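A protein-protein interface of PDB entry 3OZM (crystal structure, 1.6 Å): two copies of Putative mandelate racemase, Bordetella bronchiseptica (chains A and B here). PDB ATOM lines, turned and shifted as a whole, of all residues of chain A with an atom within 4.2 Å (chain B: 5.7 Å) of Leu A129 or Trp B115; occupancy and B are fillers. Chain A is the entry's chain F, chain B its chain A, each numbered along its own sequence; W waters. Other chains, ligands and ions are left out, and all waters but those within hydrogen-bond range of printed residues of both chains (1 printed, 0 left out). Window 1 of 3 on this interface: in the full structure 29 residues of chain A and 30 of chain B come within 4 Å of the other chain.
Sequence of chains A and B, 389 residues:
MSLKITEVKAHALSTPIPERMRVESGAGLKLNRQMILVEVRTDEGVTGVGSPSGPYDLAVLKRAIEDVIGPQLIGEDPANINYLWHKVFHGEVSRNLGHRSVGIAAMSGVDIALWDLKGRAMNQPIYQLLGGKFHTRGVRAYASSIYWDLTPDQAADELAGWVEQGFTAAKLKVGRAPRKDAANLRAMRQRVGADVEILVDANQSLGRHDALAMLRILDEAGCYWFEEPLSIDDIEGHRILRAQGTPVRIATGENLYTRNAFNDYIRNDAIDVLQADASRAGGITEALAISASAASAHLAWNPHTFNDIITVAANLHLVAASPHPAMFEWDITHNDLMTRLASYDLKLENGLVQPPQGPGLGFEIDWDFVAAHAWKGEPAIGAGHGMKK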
ATOM      1  N   TRP A 115     -43.070  10.181 -15.794  1.00  0.00           N
ATOM      2  CA  TRP A 115     -42.075  11.252 -15.808  1.00  0.00           C
ATOM      3  C   TRP A 115     -42.472  12.436 -14.904  1.00  0.00           C
ATOM      4  O   TRP A 115     -41.633  13.012 -14.194  1.00  0.00           O
ATOM      5  CB  TRP A 115     -41.810  11.701 -17.252  1.00  0.00           C
ATOM      6  CG  TRP A 115     -40.807  10.840 -17.959  1.00  0.00           C
ATOM      7  CD1 TRP A 115     -41.059   9.829 -18.851  1.00  0.00           C
ATOM      8  CD2 TRP A 115     -39.388  10.912 -17.826  1.00  0.00           C
ATOM      9  NE1 TRP A 115     -39.869   9.269 -19.282  1.00  0.00           N
ATOM     10  CE2 TRP A 115     -38.834   9.920 -18.666  1.00  0.00           C
ATOM     11  CE3 TRP A 115     -38.528  11.720 -17.072  1.00  0.00           C
ATOM     12  CZ2 TRP A 115     -37.462   9.716 -18.773  1.00  0.00           C
ATOM     13  CZ3 TRP A 115     -37.162  11.515 -17.181  1.00  0.00           C
ATOM     14  CH2 TRP A 115     -36.643  10.523 -18.028  1.00  0.00           C
ATOM     15  N   GLY A 119     -40.317  13.592 -11.699  1.00  0.00           N
ATOM     16  CA  GLY A 119     -39.951  14.982 -11.442  1.00  0.00           C
ATOM     17  C   GLY A 119     -40.456  15.484 -10.099  1.00  0.00           C
ATOM     18  O   GLY A 119     -39.738  16.152  -9.345  1.00  0.00           O
ATOM     19  N   MET A 122     -38.447  14.035  -7.257  1.00  0.00           N
ATOM     20  CA  MET A 122     -37.139  14.682  -7.167  1.00  0.00           C
ATOM     21  C   MET A 122     -37.206  16.197  -6.959  1.00  0.00           C
ATOM     22  O   MET A 122     -36.170  16.845  -6.800  1.00  0.00           O
ATOM     23  CB  MET A 122     -36.339  14.422  -8.445  1.00  0.00           C
ATOM     24  CG  MET A 122     -36.066  12.962  -8.714  1.00  0.00           C
ATOM     25  SD  MET A 122     -35.140  12.795 -10.260  1.00  0.00           S
ATOM     26  CE  MET A 122     -34.970  11.020 -10.316  1.00  0.00           C
ATOM     27  N   GLN A 124     -37.942  18.458  -9.273  1.00  0.00           N
ATOM     28  CA  GLN A 124     -37.254  19.045 -10.417  1.00  0.00           C
ATOM     29  C   GLN A 124     -38.163  19.037 -11.638  1.00  0.00           C
ATOM     30  O   GLN A 124     -38.921  18.086 -11.850  1.00  0.00           O
ATOM     31  CB  GLN A 124     -35.985  18.251 -10.756  1.00  0.00           C
ATOM     32  CG  GLN A 124     -34.881  18.324  -9.720  1.00  0.00           C
ATOM     33  CD  GLN A 124     -34.229  19.676  -9.666  1.00  0.00           C
ATOM     34  OE1 GLN A 124     -34.230  20.415 -10.644  1.00  0.00           O
ATOM     35  NE2 GLN A 124     -33.648  20.009  -8.517  1.00  0.00           N
ATOM     36  N   PRO A 125     -38.085  20.092 -12.456  1.00  0.00           N
ATOM     37  CA  PRO A 125     -38.817  20.088 -13.726  1.00  0.00           C
ATOM     38  C   PRO A 125     -38.271  18.982 -14.623  1.00  0.00           C
ATOM     39  O   PRO A 125     -37.090  18.644 -14.518  1.00  0.00           O
ATOM     40  CB  PRO A 125     -38.468  21.447 -14.341  1.00  0.00           C
ATOM     41  CG  PRO A 125     -37.901  22.268 -13.218  1.00  0.00           C
ATOM     42  CD  PRO A 125     -37.243  21.289 -12.301  1.00  0.00           C
ATOM     43  N   ILE A 126     -39.115  18.423 -15.482  1.00  0.00           N
ATOM     44  CA  ILE A 126     -38.681  17.340 -16.369  1.00  0.00           C
ATOM     45  C   ILE A 126     -37.470  17.753 -17.214  1.00  0.00           C
ATOM     46  O   ILE A 126     -36.529  16.972 -17.366  1.00  0.00           O
ATOM     47  CB  ILE A 126     -39.849  16.798 -17.247  1.00  0.00           C
ATOM     48  CG1 ILE A 126     -40.788  15.941 -16.403  1.00  0.00           C
ATOM     49  CG2 ILE A 126     -39.338  15.964 -18.440  1.00  0.00           C
ATOM     50  CD1 ILE A 126     -42.116  15.607 -17.081  1.00  0.00           C
ATOM     51  N   TYR A 127     -37.467  18.974 -17.743  1.00  0.00           N
ATOM     52  CA  TYR A 127     -36.363  19.378 -18.618  1.00  0.00           C
ATOM     53  C   TYR A 127     -35.014  19.344 -17.907  1.00  0.00           C
ATOM     54  O   TYR A 127     -33.980  19.148 -18.553  1.00  0.00           O
ATOM     55  CB  TYR A 127     -36.608  20.740 -19.275  1.00  0.00           C
ATOM     56  CG  TYR A 127     -36.511  21.940 -18.338  1.00  0.00           C
ATOM     57  CD1 TYR A 127     -35.275  22.484 -17.996  1.00  0.00           C
ATOM     58  CD2 TYR A 127     -37.656  22.540 -17.818  1.00  0.00           C
ATOM     59  CE1 TYR A 127     -35.177  23.580 -17.146  1.00  0.00           C
ATOM     60  CE2 TYR A 127     -37.565  23.646 -16.975  1.00  0.00           C
ATOM     61  CZ  TYR A 127     -36.323  24.154 -16.645  1.00  0.00           C
ATOM     62  OH  TYR A 127     -36.224  25.246 -15.809  1.00  0.00           O
ATOM     63  N   GLN A 128     -35.004  19.532 -16.583  1.00  0.00           N
ATOM     64  CA  GLN A 128     -33.740  19.439 -15.860  1.00  0.00           C
ATOM     65  C   GLN A 128     -33.235  18.003 -15.809  1.00  0.00           C
ATOM     66  O   GLN A 128     -32.032  17.770 -15.866  1.00  0.00           O
ATOM     67  CB  GLN A 128     -33.847  19.976 -14.430  1.00  0.00           C
ATOM     68  CG  GLN A 128     -34.046  21.471 -14.364  1.00  0.00           C
ATOM     69  CD  GLN A 128     -32.811  22.275 -14.762  1.00  0.00           C
ATOM     70  OE1 GLN A 128     -31.871  21.765 -15.383  1.00  0.00           O
ATOM     71  NE2 GLN A 128     -32.816  23.545 -14.403  1.00  0.00           N
ATOM     72  N   LEU A 129     -34.160  17.056 -15.676  1.00  0.00           N
ATOM     73  CA  LEU A 129     -33.804  15.637 -15.691  1.00  0.00           C
ATOM     74  C   LEU A 129     -33.155  15.279 -17.025  1.00  0.00           C
ATOM     75  O   LEU A 129     -32.236  14.464 -17.086  1.00  0.00           O
ATOM     76  CB  LEU A 129     -35.045  14.772 -15.474  1.00  0.00           C
ATOM     77  CG  LEU A 129     -35.804  15.094 -14.181  1.00  0.00           C
ATOM     78  CD1 LEU A 129     -37.033  14.211 -14.015  1.00  0.00           C
ATOM     79  CD2 LEU A 129     -34.865  14.948 -12.989  1.00  0.00           C
ATOM     80  N   LEU A 130     -33.636  15.912 -18.089  1.00  0.00           N
ATOM     81  CA  LEU A 130     -33.229  15.567 -19.453  1.00  0.00           C
ATOM     82  C   LEU A 130     -31.936  16.264 -19.883  1.00  0.00           C
ATOM     83  O   LEU A 130     -31.647  16.357 -21.076  1.00  0.00           O
ATOM     84  CB  LEU A 130     -34.359  15.902 -20.430  1.00  0.00           C
ATOM     85  CG  LEU A 130     -35.726  15.263 -20.167  1.00  0.00           C
ATOM     86  CD1 LEU A 130     -36.756  15.777 -21.181  1.00  0.00           C
ATOM     87  CD2 LEU A 130     -35.613  13.740 -20.199  1.00  0.00           C
ATOM     88  N   GLY A 131     -31.163  16.742 -18.913  1.00  0.00           N
ATOM     89  CA  GLY A 131     -29.892  17.398 -19.177  1.00  0.00           C
ATOM     90  C   GLY A 131     -29.982  18.916 -19.220  1.00  0.00           C
ATOM     91  O   GLY A 131     -29.026  19.596 -19.606  1.00  0.00           O
ATOM     92  N   ILE B  81     -26.832  21.350 -19.316  1.00  0.00           N
ATOM     93  CA  ILE B  81     -25.842  20.476 -19.940  1.00  0.00           C
ATOM     94  C   ILE B  81     -25.953  20.448 -21.469  1.00  0.00           C
ATOM     95  O   ILE B  81     -24.943  20.555 -22.178  1.00  0.00           O
ATOM     96  CB  ILE B  81     -25.918  19.056 -19.359  1.00  0.00           C
ATOM     97  CG1 ILE B  81     -25.790  19.111 -17.833  1.00  0.00           C
ATOM     98  CG2 ILE B  81     -24.836  18.162 -20.003  1.00  0.00           C
ATOM     99  CD1 ILE B  81     -25.749  17.739 -17.142  1.00  0.00           C
ATOM    100  N   VAL B 110     -15.688  16.343 -19.238  1.00  0.00           N
ATOM    101  CA  VAL B 110     -16.398  17.490 -18.670  1.00  0.00           C
ATOM    102  C   VAL B 110     -17.914  17.240 -18.618  1.00  0.00           C
ATOM    103  O   VAL B 110     -18.575  17.543 -17.638  1.00  0.00           O
ATOM    104  CB  VAL B 110     -16.071  18.741 -19.488  1.00  0.00           C
ATOM    105  CG1 VAL B 110     -16.943  19.925 -19.092  1.00  0.00           C
ATOM    106  CG2 VAL B 110     -14.600  19.074 -19.338  1.00  0.00           C
ATOM    107  N   ASP B 111     -18.465  16.654 -19.673  1.00  0.00           N
ATOM    108  CA  ASP B 111     -19.886  16.345 -19.703  1.00  0.00           C
ATOM    109  C   ASP B 111     -20.266  15.366 -18.590  1.00  0.00           C
ATOM    110  O   ASP B 111     -21.279  15.546 -17.922  1.00  0.00           O
ATOM    111  CB  ASP B 111     -20.242  15.785 -21.086  1.00  0.00           C
ATOM    112  CG  ASP B 111     -21.716  15.477 -21.248  1.00  0.00           C
ATOM    113  OD1 ASP B 111     -22.485  16.389 -21.630  1.00  0.00           O
ATOM    114  OD2 ASP B 111     -22.100  14.304 -21.021  1.00  0.00           O
ATOM    115  N   ILE B 112     -19.442  14.336 -18.386  1.00  0.00           N
ATOM    116  CA  ILE B 112     -19.671  13.421 -17.274  1.00  0.00           C
ATOM    117  C   ILE B 112     -19.657  14.196 -15.949  1.00  0.00           C
ATOM    118  O   ILE B 112     -20.501  13.981 -15.089  1.00  0.00           O
ATOM    119  CB  ILE B 112     -18.637  12.296 -17.236  1.00  0.00           C
ATOM    120  CG1 ILE B 112     -18.866  11.341 -18.417  1.00  0.00           C
ATOM    121  CG2 ILE B 112     -18.722  11.532 -15.923  1.00  0.00           C
ATOM    122  CD1 ILE B 112     -17.735  10.352 -18.651  1.00  0.00           C
ATOM    123  N   ALA B 113     -18.713  15.112 -15.807  1.00  0.00           N
ATOM    124  CA  ALA B 113     -18.623  15.887 -14.567  1.00  0.00           C
ATOM    125  C   ALA B 113     -19.893  16.727 -14.364  1.00  0.00           C
ATOM    126  O   ALA B 113     -20.378  16.886 -13.233  1.00  0.00           O
ATOM    127  CB  ALA B 113     -17.366  16.768 -14.580  1.00  0.00           C
ATOM    128  N   LEU B 114     -20.449  17.263 -15.449  1.00  0.00           N
ATOM    129  CA  LEU B 114     -21.687  18.041 -15.335  1.00  0.00           C
ATOM    130  C   LEU B 114     -22.880  17.171 -14.934  1.00  0.00           C
ATOM    131  O   LEU B 114     -23.782  17.620 -14.214  1.00  0.00           O
ATOM    132  CB  LEU B 114     -21.982  18.768 -16.643  1.00  0.00           C
ATOM    133  CG  LEU B 114     -21.021  19.887 -17.034  1.00  0.00           C
ATOM    134  CD1 LEU B 114     -21.387  20.421 -18.413  1.00  0.00           C
ATOM    135  CD2 LEU B 114     -21.076  21.011 -15.991  1.00  0.00           C
ATOM    136  N   TRP B 115     -22.896  15.930 -15.419  1.00  0.00           N
ATOM    137  CA  TRP B 115     -23.937  14.978 -15.034  1.00  0.00           C
ATOM    138  C   TRP B 115     -23.791  14.525 -13.577  1.00  0.00           C
ATOM    139  O   TRP B 115     -24.787  14.369 -12.871  1.00  0.00           O
ATOM    140  CB  TRP B 115     -23.971  13.775 -16.000  1.00  0.00           C
ATOM    141  CG  TRP B 115     -24.770  14.037 -17.239  1.00  0.00           C
ATOM    142  CD1 TRP B 115     -24.287  14.384 -18.474  1.00  0.00           C
ATOM    143  CD2 TRP B 115     -26.199  13.953 -17.377  1.00  0.00           C
ATOM    144  NE1 TRP B 115     -25.330  14.525 -19.365  1.00  0.00           N
ATOM    145  CE2 TRP B 115     -26.511  14.278 -18.714  1.00  0.00           C
ATOM    146  CE3 TRP B 115     -27.243  13.652 -16.492  1.00  0.00           C
ATOM    147  CZ2 TRP B 115     -27.822  14.286 -19.197  1.00  0.00           C
ATOM    148  CZ3 TRP B 115     -28.550  13.676 -16.967  1.00  0.00           C
ATOM    149  CH2 TRP B 115     -28.826  13.989 -18.311  1.00  0.00           C
ATOM    150  N   ASP B 116     -22.552  14.306 -13.137  1.00  0.00           N
ATOM    151  CA  ASP B 116     -22.277  13.986 -11.738  1.00  0.00           C
ATOM    152  C   ASP B 116     -22.739  15.138 -10.861  1.00  0.00           C
ATOM    153  O   ASP B 116     -23.371  14.934  -9.811  1.00  0.00           O
ATOM    154  CB  ASP B 116     -20.780  13.750 -11.544  1.00  0.00           C
ATOM    155  CG  ASP B 116     -20.438  13.292 -10.144  1.00  0.00           C
ATOM    156  OD1 ASP B 116     -21.069  12.342  -9.650  1.00  0.00           O
ATOM    157  OD2 ASP B 116     -19.514  13.882  -9.540  1.00  0.00           O
ATOM    158  N   LEU B 117     -22.438  16.354 -11.309  1.00  0.00           N
ATOM    159  CA  LEU B 117     -22.833  17.566 -10.587  1.00  0.00           C
ATOM    160  C   LEU B 117     -24.351  17.678 -10.489  1.00  0.00           C
ATOM    161  O   LEU B 117     -24.899  17.984  -9.422  1.00  0.00           O
ATOM    162  CB  LEU B 117     -22.256  18.803 -11.289  1.00  0.00           C
ATOM    163  CG  LEU B 117     -22.193  20.130 -10.511  1.00  0.00           C
ATOM    164  CD1 LEU B 117     -21.167  21.072 -11.159  1.00  0.00           C
ATOM    165  CD2 LEU B 117     -23.558  20.806 -10.428  1.00  0.00           C
ATOM    166  N   LYS B 118     -25.036  17.448 -11.609  1.00  0.00           N
ATOM    167  CA  LYS B 118     -26.491  17.516 -11.635  1.00  0.00           C
ATOM    168  C   LYS B 118     -27.098  16.491 -10.671  1.00  0.00           C
ATOM    169  O   LYS B 118     -28.018  16.806  -9.894  1.00  0.00           O
ATOM    170  CB  LYS B 118     -27.003  17.303 -13.068  1.00  0.00           C
ATOM    171  CG  LYS B 118     -28.506  17.426 -13.212  1.00  0.00           C
ATOM    172  CD  LYS B 118     -28.931  17.190 -14.669  1.00  0.00           C
ATOM    173  CE  LYS B 118     -28.712  18.446 -15.500  1.00  0.00           C
ATOM    174  NZ  LYS B 118     -29.803  19.448 -15.286  1.00  0.00           N
ATOM    175  N   GLY B 119     -26.574  15.269 -10.701  1.00  0.00           N
ATOM    176  CA  GLY B 119     -27.062  14.220  -9.822  1.00  0.00           C
ATOM    177  C   GLY B 119     -26.830  14.549  -8.356  1.00  0.00           C
ATOM    178  O   GLY B 119     -27.693  14.314  -7.503  1.00  0.00           O
ATOM    179  N   ARG B 120     -25.660  15.092  -8.058  1.00  0.00           N
ATOM    180  CA  ARG B 120     -25.350  15.474  -6.675  1.00  0.00           C
ATOM    181  C   ARG B 120     -26.238  16.634  -6.233  1.00  0.00           C
ATOM    182  O   ARG B 120     -26.701  16.658  -5.096  1.00  0.00           O
ATOM    183  CB  ARG B 120     -23.856  15.788  -6.513  1.00  0.00           C
ATOM    184  CG  ARG B 120     -23.009  14.505  -6.513  1.00  0.00           C
ATOM    185  CD  ARG B 120     -21.497  14.734  -6.478  1.00  0.00           C
ATOM    186  NE  ARG B 120     -20.795  13.612  -7.108  1.00  0.00           N
ATOM    187  CZ  ARG B 120     -20.534  12.441  -6.523  1.00  0.00           C
ATOM    188  NH1 ARG B 120     -20.902  12.224  -5.263  1.00  0.00           N
ATOM    189  NH2 ARG B 120     -19.903  11.477  -7.204  1.00  0.00           N
ATOM    190  N   MET B 122     -29.276  17.205  -7.246  1.00  0.00           N
ATOM    191  CA  MET B 122     -30.620  16.665  -7.061  1.00  0.00           C
ATOM    192  C   MET B 122     -30.684  15.544  -6.030  1.00  0.00           C
ATOM    193  O   MET B 122     -31.767  15.036  -5.737  1.00  0.00           O
ATOM    194  CB  MET B 122     -31.137  16.103  -8.392  1.00  0.00           C
ATOM    195  CG  MET B 122     -31.307  17.145  -9.470  1.00  0.00           C
ATOM    196  SD  MET B 122     -31.900  16.332 -10.970  1.00  0.00           S
ATOM    197  CE  MET B 122     -32.073  17.727 -12.066  1.00  0.00           C
ATOM    198  N   ILE B 126     -27.293   9.041 -11.323  1.00  0.00           N
ATOM    199  CA  ILE B 126     -27.544   9.406 -12.712  1.00  0.00           C
ATOM    200  C   ILE B 126     -28.564   8.482 -13.372  1.00  0.00           C
ATOM    201  O   ILE B 126     -29.436   8.945 -14.097  1.00  0.00           O
ATOM    202  CB  ILE B 126     -26.232   9.479 -13.520  1.00  0.00           C
ATOM    203  CG1 ILE B 126     -25.466  10.750 -13.138  1.00  0.00           C
ATOM    204  CG2 ILE B 126     -26.495   9.467 -15.023  1.00  0.00           C
ATOM    205  CD1 ILE B 126     -23.962  10.638 -13.389  1.00  0.00           C
ATOM    206  N   LEU B 129     -32.053   9.751 -13.197  1.00  0.00           N
ATOM    207  CA  LEU B 129     -32.345  10.882 -14.067  1.00  0.00           C
ATOM    208  C   LEU B 129     -32.703  10.411 -15.477  1.00  0.00           C
ATOM    209  O   LEU B 129     -33.504  11.039 -16.167  1.00  0.00           O
ATOM    210  CB  LEU B 129     -31.133  11.806 -14.151  1.00  0.00           C
ATOM    211  CG  LEU B 129     -30.940  12.905 -13.099  1.00  0.00           C
ATOM    212  CD1 LEU B 129     -31.354  12.463 -11.706  1.00  0.00           C
ATOM    213  CD2 LEU B 129     -29.503  13.412 -13.116  1.00  0.00           C
ATOM    214  N   LEU B 130     -32.111   9.294 -15.881  1.00  0.00           N
ATOM    215  CA  LEU B 130     -32.213   8.798 -17.259  1.00  0.00           C
ATOM    216  C   LEU B 130     -33.423   7.913 -17.468  1.00  0.00           C
ATOM    217  O   LEU B 130     -33.460   7.127 -18.410  1.00  0.00           O
ATOM    218  CB  LEU B 130     -30.964   7.988 -17.619  1.00  0.00           C
ATOM    219  CG  LEU B 130     -29.627   8.705 -17.467  1.00  0.00           C
ATOM    220  CD1 LEU B 130     -28.506   7.739 -17.866  1.00  0.00           C
ATOM    221  CD2 LEU B 130     -29.598   9.981 -18.293  1.00  0.00           C
ATOM    222  N   ILE B 284     -21.847  11.592 -21.512  1.00  0.00           N
ATOM    223  CA  ILE B 284     -23.124  10.932 -21.255  1.00  0.00           C
ATOM    224  C   ILE B 284     -24.181  11.456 -22.226  1.00  0.00           C
ATOM    225  O   ILE B 284     -24.976  10.689 -22.779  1.00  0.00           O
ATOM    226  CB  ILE B 284     -23.545  11.107 -19.778  1.00  0.00           C
ATOM    227  CG1 ILE B 284     -22.755  10.128 -18.898  1.00  0.00           C
ATOM    228  CG2 ILE B 284     -25.063  10.927 -19.606  1.00  0.00           C
ATOM    229  CD1 ILE B 284     -22.899  10.390 -17.374  1.00  0.00           C
ATOM    230  N   THR B 285     -24.169  12.761 -22.466  1.00  0.00           N
ATOM    231  CA  THR B 285     -25.121  13.366 -23.384  1.00  0.00           C
ATOM    232  C   THR B 285     -25.076  12.698 -24.760  1.00  0.00           C
ATOM    233  O   THR B 285     -26.110  12.333 -25.337  1.00  0.00           O
ATOM    234  CB  THR B 285     -24.828  14.867 -23.528  1.00  0.00           C
ATOM    235  OG1 THR B 285     -24.851  15.469 -22.217  1.00  0.00           O
ATOM    236  CG2 THR B 285     -25.867  15.537 -24.413  1.00  0.00           C
ATOM    237  N   LEU B 288     -26.005   8.732 -24.725  1.00  0.00           N
ATOM    238  CA  LEU B 288     -27.461   8.556 -24.677  1.00  0.00           C
ATOM    239  C   LEU B 288     -28.086   8.593 -26.082  1.00  0.00           C
ATOM    240  O   LEU B 288     -28.949   7.778 -26.429  1.00  0.00           O
ATOM    241  CB  LEU B 288     -28.102   9.649 -23.824  1.00  0.00           C
ATOM    242  CG  LEU B 288     -27.993   9.507 -22.308  1.00  0.00           C
ATOM    243  CD1 LEU B 288     -28.453  10.791 -21.629  1.00  0.00           C
ATOM    244  CD2 LEU B 288     -28.810   8.309 -21.836  1.00  0.00           C
ATOM    245  N   GLY B 360     -25.302  11.282  -8.230  1.00  0.00           N
ATOM    246  CA  GLY B 360     -24.392  11.454  -9.357  1.00  0.00           C
ATOM    247  C   GLY B 360     -23.839  10.123  -9.827  1.00  0.00           C
ATOM    248  O   GLY B 360     -24.600   9.171 -10.008  1.00  0.00           O
ATOM    249  N   LEU B 361     -22.521  10.049 -10.019  1.00  0.00           N
ATOM    250  CA  LEU B 361     -21.872   8.785 -10.359  1.00  0.00           C
ATOM    251  C   LEU B 361     -22.053   7.759  -9.257  1.00  0.00           C
ATOM    252  O   LEU B 361     -21.948   6.559  -9.495  1.00  0.00           O
ATOM    253  CB  LEU B 361     -20.388   9.000 -10.656  1.00  0.00           C
ATOM    254  CG  LEU B 361     -20.110   9.815 -11.922  1.00  0.00           C
ATOM    255  CD1 LEU B 361     -18.681  10.357 -11.931  1.00  0.00           C
ATOM    256  CD2 LEU B 361     -20.397   8.985 -13.180  1.00  0.00           C
HETATM  257  O   HOH W   1     -32.660  12.045 -18.558  1.00  0.00           O
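Of the printed residues of chain B, Gln A128 touches Lys B118 (2.8 Å) and Met B122 (3.7 Å). Printed residues of chain B within 4 Å of Leu A129: Trp B115, Met B122 and Leu B129. Of the printed residues of chain B, Gly A131 touches Ile B81 (2.8 Å), Trp B115 (3.7 Å) and Lys B118 (3.96 Å). Of the printed residues of chain A, Trp B115 touches Leu A129 and Gly A131. Of the printed residues of chain A, Lys B118 touches Gln A128 (2.8 Å) and Gly A131 (3.96 Å). Of the printed residues of chain A, Met B122 touches Gln A124, Gln A128 and Leu A129. The nearest printed residue of chain B that does not touch Leu A129 is Lys B118 (4.9 Å). The nearest printed residue of chain A that does not touch Trp B115 is Leu A130 (4.2 Å). The nearest printed residue of chain B that does not touch Gln A128 is Trp B115 (5.5 Å).
Trp A115 touches Leu B129, and with the chains exchanged Leu A129 touches Trp B115. Leu A129 touches Met B122, but with the chains exchanged Met A122 does not touch Leu B129 (4.1 Å). Leu A129 touches its own counterpart, Leu B129. 6 positions are printed for both chains.
OG1 of Thr B285 is in hydrogen-bond range of NE1 of Trp B115. The backbone NH (N) of Gln A124 lies within hydrogen-bond range of the backbone carbonyl oxygen (O) of Gly A119, 2.9 Å away.
Printed residues of chain A that touch a printed residue of chain B: Trp A115, Gln A124, Gln A128, Leu A129 and Gly A131. Among the printed residues, no Asp or Glu carboxylate lies within 4 Å of a Lys or Arg side-chain nitrogen of the other chain.
The backbone carbonyl oxygen (O) of Gln A128 lies within hydrogen-bond range of the side-chain amino group (NZ) of Lys B118 (2.8 Å). The backbone NH of Ile B81 sits at hydrogen-bond distance from the backbone carbonyl oxygen of Gly A131 (2.8 Å).
Trp A115 touches Leu B129 (CH2 to O, 3.7 Å). Met B122 touches Gln A124. Gln A128 touches Met B122. Leu A129 touches Trp B115 (O to CH2, 3.7 Å). Leu A129 touches Met B122. Leu A129 touches Leu B129 (O to O, 3.8 Å). Trp B115 touches Gly A131 (CH2 to N, 3.7 Å). Gly A131 touches Lys B118.
Water W1 lies within hydrogen-bond range of O of Leu B129 (2.7 Å) and O of Leu A129 (2.9 Å).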
